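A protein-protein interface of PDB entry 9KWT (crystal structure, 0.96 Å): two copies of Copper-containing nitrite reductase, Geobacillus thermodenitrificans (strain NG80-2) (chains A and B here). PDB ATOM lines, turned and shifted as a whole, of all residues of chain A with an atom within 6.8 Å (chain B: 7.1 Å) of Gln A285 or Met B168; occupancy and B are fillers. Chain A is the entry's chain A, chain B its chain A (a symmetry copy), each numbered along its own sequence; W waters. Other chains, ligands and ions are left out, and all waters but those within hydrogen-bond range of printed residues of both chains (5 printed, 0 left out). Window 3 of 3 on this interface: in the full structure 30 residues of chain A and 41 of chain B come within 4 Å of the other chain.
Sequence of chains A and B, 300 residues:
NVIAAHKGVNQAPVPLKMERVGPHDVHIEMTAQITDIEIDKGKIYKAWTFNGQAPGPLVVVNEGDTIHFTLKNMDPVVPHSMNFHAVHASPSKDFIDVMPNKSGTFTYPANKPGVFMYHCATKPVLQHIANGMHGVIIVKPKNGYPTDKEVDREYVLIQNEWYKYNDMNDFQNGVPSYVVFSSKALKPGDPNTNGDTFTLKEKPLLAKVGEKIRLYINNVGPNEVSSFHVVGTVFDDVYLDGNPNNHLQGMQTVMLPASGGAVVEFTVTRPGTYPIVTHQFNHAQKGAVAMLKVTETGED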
ATOM      1  N   VAL A 179     -26.801   4.502 -23.142  1.00  0.00           N
ATOM      2  CA  VAL A 179     -26.896   3.215 -23.812  1.00  0.00           C
ATOM      3  C   VAL A 179     -26.694   2.191 -22.708  1.00  0.00           C
ATOM      4  O   VAL A 179     -25.828   2.386 -21.855  1.00  0.00           O
ATOM      5  CB  VAL A 179     -25.876   3.073 -24.964  1.00  0.00           C
ATOM      6  CG1 VAL A 179     -26.131   1.780 -25.721  1.00  0.00           C
ATOM      7  CG2 VAL A 179     -25.962   4.267 -25.910  1.00  0.00           C
ATOM      8  N   THR A 278     -20.658  -2.965 -25.293  1.00  0.00           N
ATOM      9  CA  THR A 278     -20.524  -2.614 -26.699  1.00  0.00           C
ATOM     10  C   THR A 278     -19.194  -1.882 -26.853  1.00  0.00           C
ATOM     11  O   THR A 278     -18.877  -0.982 -26.071  1.00  0.00           O
ATOM     12  CB  THR A 278     -21.690  -1.799 -27.255  1.00  0.00           C
ATOM     13  OG1 THR A 278     -21.338  -1.472 -28.606  1.00  0.00           O
ATOM     14  CG2 THR A 278     -21.960  -0.540 -26.458  1.00  0.00           C
ATOM     15  N   GLN A 280     -18.223   0.055 -29.130  1.00  0.00           N
ATOM     16  CA  GLN A 280     -18.385   1.450 -29.510  1.00  0.00           C
ATOM     17  C   GLN A 280     -18.322   2.224 -28.202  1.00  0.00           C
ATOM     18  O   GLN A 280     -19.298   2.276 -27.445  1.00  0.00           O
ATOM     19  CB  GLN A 280     -19.695   1.616 -30.264  1.00  0.00           C
ATOM     20  CG  GLN A 280     -19.626   0.934 -31.632  1.00  0.00           C
ATOM     21  CD  GLN A 280     -20.977   0.556 -32.209  1.00  0.00           C
ATOM     22  OE1 GLN A 280     -21.220  -0.615 -32.527  1.00  0.00           O
ATOM     23  NE2 GLN A 280     -21.858   1.526 -32.357  1.00  0.00           N
ATOM     24  N   PHE A 281     -17.128   2.711 -27.865  1.00  0.00           N
ATOM     25  CA  PHE A 281     -16.861   3.062 -26.475  1.00  0.00           C
ATOM     26  C   PHE A 281     -17.551   4.334 -26.019  1.00  0.00           C
ATOM     27  O   PHE A 281     -17.697   4.539 -24.808  1.00  0.00           O
ATOM     28  CB  PHE A 281     -15.350   3.020 -26.143  1.00  0.00           C
ATOM     29  CG  PHE A 281     -15.011   1.826 -25.297  1.00  0.00           C
ATOM     30  CD1 PHE A 281     -15.223   1.875 -23.928  1.00  0.00           C
ATOM     31  CD2 PHE A 281     -14.619   0.627 -25.868  1.00  0.00           C
ATOM     32  CE1 PHE A 281     -15.036   0.745 -23.147  1.00  0.00           C
ATOM     33  CE2 PHE A 281     -14.420  -0.496 -25.088  1.00  0.00           C
ATOM     34  CZ  PHE A 281     -14.632  -0.439 -23.728  1.00  0.00           C
ATOM     35  N   ASN A 282     -18.018   5.163 -26.943  1.00  0.00           N
ATOM     36  CA  ASN A 282     -18.876   6.270 -26.542  1.00  0.00           C
ATOM     37  C   ASN A 282     -20.155   5.755 -25.895  1.00  0.00           C
ATOM     38  O   ASN A 282     -20.636   6.323 -24.908  1.00  0.00           O
ATOM     39  CB  ASN A 282     -19.176   7.237 -27.703  1.00  0.00           C
ATOM     40  CG  ASN A 282     -19.674   6.596 -29.000  1.00  0.00           C
ATOM     41  OD1 ASN A 282     -19.776   5.404 -29.175  1.00  0.00           O
ATOM     42  ND2 ASN A 282     -19.981   7.470 -29.950  1.00  0.00           N
ATOM     43  N   HIS A 283     -20.713   4.676 -26.439  1.00  0.00           N
ATOM     44  CA  HIS A 283     -21.905   4.063 -25.867  1.00  0.00           C
ATOM     45  C   HIS A 283     -21.594   3.356 -24.554  1.00  0.00           C
ATOM     46  O   HIS A 283     -22.379   3.435 -23.604  1.00  0.00           O
ATOM     47  CB  HIS A 283     -22.511   3.091 -26.872  1.00  0.00           C
ATOM     48  CG  HIS A 283     -22.938   3.737 -28.145  1.00  0.00           C
ATOM     49  ND1 HIS A 283     -23.241   2.994 -29.260  1.00  0.00           N
ATOM     50  CD2 HIS A 283     -23.096   5.045 -28.478  1.00  0.00           C
ATOM     51  CE1 HIS A 283     -23.563   3.828 -30.229  1.00  0.00           C
ATOM     52  NE2 HIS A 283     -23.486   5.077 -29.787  1.00  0.00           N
ATOM     53  N   ALA A 284     -20.454   2.658 -24.481  1.00  0.00           N
ATOM     54  CA  ALA A 284     -20.038   2.052 -23.224  1.00  0.00           C
ATOM     55  C   ALA A 284     -19.906   3.106 -22.130  1.00  0.00           C
ATOM     56  O   ALA A 284     -20.361   2.903 -20.998  1.00  0.00           O
ATOM     57  CB  ALA A 284     -18.724   1.300 -23.428  1.00  0.00           C
ATOM     58  N   GLN A 285     -19.302   4.252 -22.463  1.00  0.00           N
ATOM     59  CA  GLN A 285     -19.133   5.314 -21.483  1.00  0.00           C
ATOM     60  C   GLN A 285     -20.468   5.852 -20.998  1.00  0.00           C
ATOM     61  O   GLN A 285     -20.585   6.282 -19.845  1.00  0.00           O
ATOM     62  CB  GLN A 285     -18.253   6.415 -22.071  1.00  0.00           C
ATOM     63  CG  GLN A 285     -18.126   7.623 -21.163  1.00  0.00           C
ATOM     64  CD  GLN A 285     -17.319   7.338 -19.909  1.00  0.00           C
ATOM     65  OE1 GLN A 285     -16.523   6.396 -19.834  1.00  0.00           O
ATOM     66  NE2 GLN A 285     -17.605   8.113 -18.865  1.00  0.00           N
ATOM     67  N   LYS A 286     -21.475   5.850 -21.870  1.00  0.00           N
ATOM     68  CA  LYS A 286     -22.812   6.335 -21.565  1.00  0.00           C
ATOM     69  C   LYS A 286     -23.726   5.232 -21.018  1.00  0.00           C
ATOM     70  O   LYS A 286     -24.949   5.397 -21.001  1.00  0.00           O
ATOM     71  CB  LYS A 286     -23.401   7.075 -22.770  1.00  0.00           C
ATOM     72  CG  LYS A 286     -22.648   8.373 -23.051  1.00  0.00           C
ATOM     73  CD  LYS A 286     -23.288   9.266 -24.096  1.00  0.00           C
ATOM     74  CE  LYS A 286     -23.132   8.739 -25.507  1.00  0.00           C
ATOM     75  NZ  LYS A 286     -23.643   9.719 -26.517  1.00  0.00           N
ATOM     76  N   GLY A 287     -23.138   4.148 -20.507  1.00  0.00           N
ATOM     77  CA  GLY A 287     -23.847   3.197 -19.681  1.00  0.00           C
ATOM     78  C   GLY A 287     -23.701   1.739 -20.048  1.00  0.00           C
ATOM     79  O   GLY A 287     -24.040   0.880 -19.224  1.00  0.00           O
ATOM     80  N   ALA A 288     -23.240   1.441 -21.267  1.00  0.00           N
ATOM     81  CA  ALA A 288     -23.385   0.101 -21.839  1.00  0.00           C
ATOM     82  C   ALA A 288     -22.198  -0.786 -21.466  1.00  0.00           C
ATOM     83  O   ALA A 288     -21.420  -1.247 -22.300  1.00  0.00           O
ATOM     84  CB  ALA A 288     -23.602   0.175 -23.339  1.00  0.00           C
ATOM     85  N   VAL A 289     -22.120  -1.037 -20.158  1.00  0.00           N
ATOM     86  CA  VAL A 289     -21.183  -1.976 -19.552  1.00  0.00           C
ATOM     87  C   VAL A 289     -21.956  -2.755 -18.493  1.00  0.00           C
ATOM     88  O   VAL A 289     -22.529  -2.161 -17.573  1.00  0.00           O
ATOM     89  CB  VAL A 289     -19.957  -1.296 -18.918  1.00  0.00           C
ATOM     90  CG1 VAL A 289     -19.038  -2.350 -18.296  1.00  0.00           C
ATOM     91  CG2 VAL A 289     -19.208  -0.448 -19.938  1.00  0.00           C
ATOM     92  N   ASN B   1      -8.986  20.017 -20.128  1.00  0.00           N
ATOM     93  CA  ASN B   1      -8.534  18.847 -20.875  1.00  0.00           C
ATOM     94  C   ASN B   1      -7.007  18.743 -20.902  1.00  0.00           C
ATOM     95  O   ASN B   1      -6.453  17.766 -21.395  1.00  0.00           O
ATOM     96  CB  ASN B   1      -9.082  18.883 -22.306  1.00  0.00           C
ATOM     97  CG  ASN B   1     -10.565  19.190 -22.354  1.00  0.00           C
ATOM     98  OD1 ASN B   1     -11.331  18.757 -21.491  1.00  0.00           O
ATOM     99  ND2 ASN B   1     -10.984  19.931 -23.376  1.00  0.00           N
ATOM    100  N   LYS B 123      -9.882   2.931 -16.513  1.00  0.00           N
ATOM    101  CA  LYS B 123     -11.093   3.743 -16.532  1.00  0.00           C
ATOM    102  C   LYS B 123     -10.726   5.228 -16.560  1.00  0.00           C
ATOM    103  O   LYS B 123      -9.825   5.660 -15.829  1.00  0.00           O
ATOM    104  CB  LYS B 123     -11.934   3.454 -15.284  1.00  0.00           C
ATOM    105  CG  LYS B 123     -13.169   4.347 -15.109  1.00  0.00           C
ATOM    106  CD  LYS B 123     -14.258   3.668 -14.268  1.00  0.00           C
ATOM    107  CE  LYS B 123     -15.414   4.611 -13.966  1.00  0.00           C
ATOM    108  NZ  LYS B 123     -15.430   5.077 -12.554  1.00  0.00           N
ATOM    109  N   PRO B 124     -11.416   6.044 -17.375  1.00  0.00           N
ATOM    110  CA  PRO B 124     -12.431   5.673 -18.374  1.00  0.00           C
ATOM    111  C   PRO B 124     -11.775   5.097 -19.617  1.00  0.00           C
ATOM    112  O   PRO B 124     -10.906   5.737 -20.225  1.00  0.00           O
ATOM    113  CB  PRO B 124     -13.130   6.998 -18.707  1.00  0.00           C
ATOM    114  CG  PRO B 124     -12.543   8.014 -17.817  1.00  0.00           C
ATOM    115  CD  PRO B 124     -11.253   7.498 -17.296  1.00  0.00           C
ATOM    116  N   VAL B 125     -12.189   3.891 -20.000  1.00  0.00           N
ATOM    117  CA  VAL B 125     -11.539   3.226 -21.122  1.00  0.00           C
ATOM    118  C   VAL B 125     -11.670   4.052 -22.400  1.00  0.00           C
ATOM    119  O   VAL B 125     -10.731   4.134 -23.198  1.00  0.00           O
ATOM    120  CB  VAL B 125     -12.081   1.794 -21.277  1.00  0.00           C
ATOM    121  CG1 VAL B 125     -11.518   1.126 -22.520  1.00  0.00           C
ATOM    122  CG2 VAL B 125     -11.742   0.968 -20.031  1.00  0.00           C
ATOM    123  N   LEU B 126     -12.824   4.684 -22.615  1.00  0.00           N
ATOM    124  CA  LEU B 126     -12.981   5.548 -23.786  1.00  0.00           C
ATOM    125  C   LEU B 126     -11.878   6.589 -23.867  1.00  0.00           C
ATOM    126  O   LEU B 126     -11.379   6.893 -24.951  1.00  0.00           O
ATOM    127  CB  LEU B 126     -14.338   6.250 -23.735  1.00  0.00           C
ATOM    128  CG  LEU B 126     -14.568   7.355 -24.768  1.00  0.00           C
ATOM    129  CD1 LEU B 126     -14.527   6.825 -26.198  1.00  0.00           C
ATOM    130  CD2 LEU B 126     -15.893   8.032 -24.476  1.00  0.00           C
ATOM    131  N   GLN B 127     -11.520   7.188 -22.732  1.00  0.00           N
ATOM    132  CA  GLN B 127     -10.488   8.224 -22.725  1.00  0.00           C
ATOM    133  C   GLN B 127      -9.135   7.661 -23.146  1.00  0.00           C
ATOM    134  O   GLN B 127      -8.407   8.272 -23.941  1.00  0.00           O
ATOM    135  CB  GLN B 127     -10.407   8.853 -21.332  1.00  0.00           C
ATOM    136  CG  GLN B 127      -9.467  10.027 -21.257  1.00  0.00           C
ATOM    137  CD  GLN B 127      -9.491  10.713 -19.911  1.00  0.00           C
ATOM    138  OE1 GLN B 127      -9.967  10.150 -18.924  1.00  0.00           O
ATOM    139  NE2 GLN B 127      -8.986  11.937 -19.868  1.00  0.00           N
ATOM    140  N   HIS B 128      -8.766   6.505 -22.591  1.00  0.00           N
ATOM    141  CA  HIS B 128      -7.468   5.927 -22.896  1.00  0.00           C
ATOM    142  C   HIS B 128      -7.401   5.453 -24.344  1.00  0.00           C
ATOM    143  O   HIS B 128      -6.379   5.666 -25.012  1.00  0.00           O
ATOM    144  CB  HIS B 128      -7.149   4.812 -21.909  1.00  0.00           C
ATOM    145  CG  HIS B 128      -6.839   5.321 -20.540  1.00  0.00           C
ATOM    146  ND1 HIS B 128      -5.556   5.346 -20.037  1.00  0.00           N
ATOM    147  CD2 HIS B 128      -7.640   5.876 -19.598  1.00  0.00           C
ATOM    148  CE1 HIS B 128      -5.588   5.861 -18.825  1.00  0.00           C
ATOM    149  NE2 HIS B 128      -6.834   6.203 -18.540  1.00  0.00           N
ATOM    150  N   ALA B 130      -9.342   6.609 -26.927  1.00  0.00           N
ATOM    151  CA  ALA B 130      -9.431   7.745 -27.837  1.00  0.00           C
ATOM    152  C   ALA B 130      -8.130   8.531 -27.889  1.00  0.00           C
ATOM    153  O   ALA B 130      -7.773   9.075 -28.937  1.00  0.00           O
ATOM    154  CB  ALA B 130     -10.581   8.662 -27.452  1.00  0.00           C
ATOM    155  N   LYS B 164     -11.240  15.789 -30.667  1.00  0.00           N
ATOM    156  CA  LYS B 164     -10.649  16.932 -29.991  1.00  0.00           C
ATOM    157  C   LYS B 164      -9.826  16.466 -28.798  1.00  0.00           C
ATOM    158  O   LYS B 164     -10.200  15.526 -28.098  1.00  0.00           O
ATOM    159  CB  LYS B 164     -11.710  17.954 -29.576  1.00  0.00           C
ATOM    160  CG  LYS B 164     -12.536  18.515 -30.718  1.00  0.00           C
ATOM    161  CD  LYS B 164     -13.784  19.238 -30.211  1.00  0.00           C
ATOM    162  CE  LYS B 164     -14.648  19.713 -31.356  1.00  0.00           C
ATOM    163  NZ  LYS B 164     -15.657  20.688 -30.899  1.00  0.00           N
ATOM    164  N   TYR B 165      -8.716  17.150 -28.555  1.00  0.00           N
ATOM    165  CA  TYR B 165      -7.686  16.625 -27.671  1.00  0.00           C
ATOM    166  C   TYR B 165      -8.210  16.379 -26.258  1.00  0.00           C
ATOM    167  O   TYR B 165      -8.611  17.312 -25.556  1.00  0.00           O
ATOM    168  CB  TYR B 165      -6.492  17.580 -27.607  1.00  0.00           C
ATOM    169  CG  TYR B 165      -5.397  16.957 -26.805  1.00  0.00           C
ATOM    170  CD1 TYR B 165      -4.662  15.919 -27.341  1.00  0.00           C
ATOM    171  CD2 TYR B 165      -5.147  17.342 -25.494  1.00  0.00           C
ATOM    172  CE1 TYR B 165      -3.689  15.286 -26.605  1.00  0.00           C
ATOM    173  CE2 TYR B 165      -4.182  16.711 -24.752  1.00  0.00           C
ATOM    174  CZ  TYR B 165      -3.452  15.686 -25.304  1.00  0.00           C
ATOM    175  OH  TYR B 165      -2.485  15.076 -24.558  1.00  0.00           O
ATOM    176  N   ASN B 166      -8.124  15.124 -25.812  1.00  0.00           N
ATOM    177  CA  ASN B 166      -8.445  14.756 -24.431  1.00  0.00           C
ATOM    178  C   ASN B 166      -9.772  15.356 -23.958  1.00  0.00           C
ATOM    179  O   ASN B 166      -9.895  15.767 -22.809  1.00  0.00           O
ATOM    180  CB  ASN B 166      -7.319  15.117 -23.463  1.00  0.00           C
ATOM    181  CG  ASN B 166      -7.470  14.413 -22.141  1.00  0.00           C
ATOM    182  OD1 ASN B 166      -7.858  13.245 -22.093  1.00  0.00           O
ATOM    183  ND2 ASN B 166      -7.165  15.105 -21.061  1.00  0.00           N
ATOM    184  N   ASP B 167     -10.771  15.370 -24.836  1.00  0.00           N
ATOM    185  CA  ASP B 167     -12.051  16.037 -24.582  1.00  0.00           C
ATOM    186  C   ASP B 167     -13.122  14.966 -24.431  1.00  0.00           C
ATOM    187  O   ASP B 167     -13.644  14.454 -25.421  1.00  0.00           O
ATOM    188  CB  ASP B 167     -12.348  16.987 -25.734  1.00  0.00           C
ATOM    189  CG  ASP B 167     -13.674  17.698 -25.607  1.00  0.00           C
ATOM    190  OD1 ASP B 167     -14.519  17.297 -24.780  1.00  0.00           O
ATOM    191  OD2 ASP B 167     -13.868  18.654 -26.389  1.00  0.00           O
ATOM    192  N   MET B 168     -13.444  14.611 -23.187  1.00  0.00           N
ATOM    193  CA  MET B 168     -14.385  13.517 -22.945  1.00  0.00           C
ATOM    194  C   MET B 168     -15.772  13.820 -23.482  1.00  0.00           C
ATOM    195  O   MET B 168     -16.492  12.898 -23.875  1.00  0.00           O
ATOM    196  CB  MET B 168     -14.439  13.185 -21.455  1.00  0.00           C
ATOM    197  CG  MET B 168     -13.381  12.170 -21.029  1.00  0.00           C
ATOM    198  SD  MET B 168     -13.654  10.506 -21.680  1.00  0.00           S
ATOM    199  CE  MET B 168     -14.849   9.886 -20.520  1.00  0.00           C
ATOM    200  N   ASN B 169     -16.196  15.081 -23.485  1.00  0.00           N
ATOM    201  CA  ASN B 169     -17.485  15.393 -24.079  1.00  0.00           C
ATOM    202  C   ASN B 169     -17.481  15.054 -25.561  1.00  0.00           C
ATOM    203  O   ASN B 169     -18.416  14.429 -26.081  1.00  0.00           O
ATOM    204  CB  ASN B 169     -17.842  16.858 -23.876  1.00  0.00           C
ATOM    205  CG  ASN B 169     -19.182  17.173 -24.447  1.00  0.00           C
ATOM    206  OD1 ASN B 169     -20.177  16.544 -24.094  1.00  0.00           O
ATOM    207  ND2 ASN B 169     -19.200  18.051 -25.437  1.00  0.00           N
ATOM    208  N   ASP B 170     -16.430  15.472 -26.267  1.00  0.00           N
ATOM    209  CA  ASP B 170     -16.317  15.157 -27.686  1.00  0.00           C
ATOM    210  C   ASP B 170     -16.197  13.659 -27.909  1.00  0.00           C
ATOM    211  O   ASP B 170     -16.804  13.103 -28.834  1.00  0.00           O
ATOM    212  CB  ASP B 170     -15.123  15.903 -28.287  1.00  0.00           C
ATOM    213  CG  ASP B 170     -15.154  15.944 -29.795  1.00  0.00           C
ATOM    214  OD1 ASP B 170     -16.179  16.408 -30.344  1.00  0.00           O
ATOM    215  OD2 ASP B 170     -14.149  15.549 -30.422  1.00  0.00           O
ATOM    216  N   PHE B 171     -15.404  12.985 -27.077  1.00  0.00           N
ATOM    217  CA  PHE B 171     -15.231  11.549 -27.239  1.00  0.00           C
ATOM    218  C   PHE B 171     -16.571  10.821 -27.182  1.00  0.00           C
ATOM    219  O   PHE B 171     -16.776   9.825 -27.888  1.00  0.00           O
ATOM    220  CB  PHE B 171     -14.335  10.962 -26.139  1.00  0.00           C
ATOM    221  CG  PHE B 171     -12.883  11.408 -26.130  1.00  0.00           C
ATOM    222  CD1 PHE B 171     -12.299  12.119 -27.162  1.00  0.00           C
ATOM    223  CD2 PHE B 171     -12.085  11.031 -25.062  1.00  0.00           C
ATOM    224  CE1 PHE B 171     -10.957  12.464 -27.110  1.00  0.00           C
ATOM    225  CE2 PHE B 171     -10.742  11.380 -25.013  1.00  0.00           C
ATOM    226  CZ  PHE B 171     -10.179  12.083 -26.045  1.00  0.00           C
ATOM    227  N   GLN B 172     -17.466  11.278 -26.294  1.00  0.00           N
ATOM    228  CA  GLN B 172     -18.751  10.621 -26.051  1.00  0.00           C
ATOM    229  C   GLN B 172     -19.809  11.023 -27.063  1.00  0.00           C
ATOM    230  O   GLN B 172     -20.655  10.201 -27.438  1.00  0.00           O
ATOM    231  CB  GLN B 172     -19.290  11.002 -24.669  1.00  0.00           C
ATOM    232  CG  GLN B 172     -18.613  10.300 -23.524  1.00  0.00           C
ATOM    233  CD  GLN B 172     -19.077  10.826 -22.188  1.00  0.00           C
ATOM    234  OE1 GLN B 172     -20.128  10.449 -21.663  1.00  0.00           O
ATOM    235  NE2 GLN B 172     -18.273  11.693 -21.621  1.00  0.00           N
ATOM    236  N   ASN B 173     -19.811  12.299 -27.450  1.00  0.00           N
ATOM    237  CA  ASN B 173     -20.949  12.929 -28.109  1.00  0.00           C
ATOM    238  C   ASN B 173     -20.660  13.532 -29.470  1.00  0.00           C
ATOM    239  O   ASN B 173     -21.618  13.933 -30.145  1.00  0.00           O
ATOM    240  CB  ASN B 173     -21.536  14.020 -27.202  1.00  0.00           C
ATOM    241  CG  ASN B 173     -22.065  13.453 -25.909  1.00  0.00           C
ATOM    242  OD1 ASN B 173     -22.803  12.480 -25.913  1.00  0.00           O
ATOM    243  ND2 ASN B 173     -21.682  14.046 -24.790  1.00  0.00           N
ATOM    244  N   GLY B 174     -19.399  13.644 -29.877  1.00  0.00           N
ATOM    245  CA  GLY B 174     -19.039  14.346 -31.087  1.00  0.00           C
ATOM    246  C   GLY B 174     -18.666  13.414 -32.224  1.00  0.00           C
ATOM    247  O   GLY B 174     -18.225  12.288 -32.019  1.00  0.00           O
HETATM  248  O   HOH W   1     -15.325   4.271 -21.240  1.00  0.00           O
HETATM  249  O   HOH W   2     -21.210  10.432 -30.426  1.00  0.00           O
HETATM  250  O   HOH W   3     -18.433  10.310 -30.198  1.00  0.00           O
HETATM  251  O   HOH W   4     -19.910  10.026 -19.096  1.00  0.00           O
HETATM  252  O   HOH W   5     -23.026   8.845 -28.992  1.00  0.00           O
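Printed residues of chain B within 4 Å of Gln A285: Pro B124, Leu B126, Met B168 and Gln B172. Printed residues of chain A within 4 Å of Val B125: Phe A281 (3.6 Å). Of the printed residues of chain A, Met B168 touches Gln A285. Of the printed residues of chain A, Asn B173 touches Lys A286 (2.9 Å). Gly B174 touches none of the printed residues of chain A. The nearest printed residue of chain A that does not touch Met B168 is Asn A282 (7.3 Å).
No position is printed for both chains. Of the 11 pairs that touch across the chains among the printed residues, none has its exchanged pair printed and touching as well.
The side-chain amino group (NZ) of Lys A286 lies within hydrogen-bond range of the side-chain amide oxygen (OD1) of Asn B173, at 2.9 Å. NZ of Lys A286 is in hydrogen-bond range of O of Gln B172, at 3.2 Å.
O of Met B168 lies within hydrogen-bond range of NE2 of Gln B172 (3.1 Å). The backbone NH (N) of Val A179 sits at hydrogen-bond distance from the backbone carbonyl oxygen (O) of Lys A286. The side-chain amide nitrogen (ND2) of Asn B173 lies within hydrogen-bond range of the side-chain amide oxygen (OD1) of Asn B169 (3.0 Å).
Water W4 lies within hydrogen-bond range of OE1 of Gln B172 (2.6 Å) and NE2 of Gln A285 (3.0 Å). Water W5 lies within hydrogen-bond range of the side-chain amino group (NZ) of Lys A286, the backbone carbonyl oxygen (O) of Gln B172 and the side-chain amide nitrogen (ND2) of Asn A282. Water W3 lies within hydrogen-bond range of the backbone carbonyl oxygen (O) of Gly B174 (2.7 Å), the backbone carbonyl oxygen (O) of Phe B171 (2.9 Å) and the side-chain amide nitrogen (ND2) of Asn A282 (3.2 Å). Water W1 lies within hydrogen-bond range of OE1 of Gln A285 (2.8 Å), N of Leu B126 (2.9 Å) and N of Val B125 (3.4 Å). Water W2 lies within hydrogen-bond range of the backbone carbonyl oxygen of Gln B172 (3.0 Å) and the side-chain amide nitrogen of Asn A282 (3.2 Å).
Hydrophobic or aromatic side chains of chain B within 4 Å of the printed part of chain A: Pro B124, Val B125, Leu B126 and Met B168. Of the 12 printed residues of chain A, 4 touch a printed residue of chain B.
Among the printed residues, pairs that only touch across the chains: Asn A282 with Gln B172, Gln A285 with Gln B172, Asn A282 with Phe B171, Phe A281 with Val B125, Gln A285 with Met B168, Gln A285 with Pro B124, Gln A285 with Leu B126, Phe A281 with Leu B126 and Asn A282 with Leu B126.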
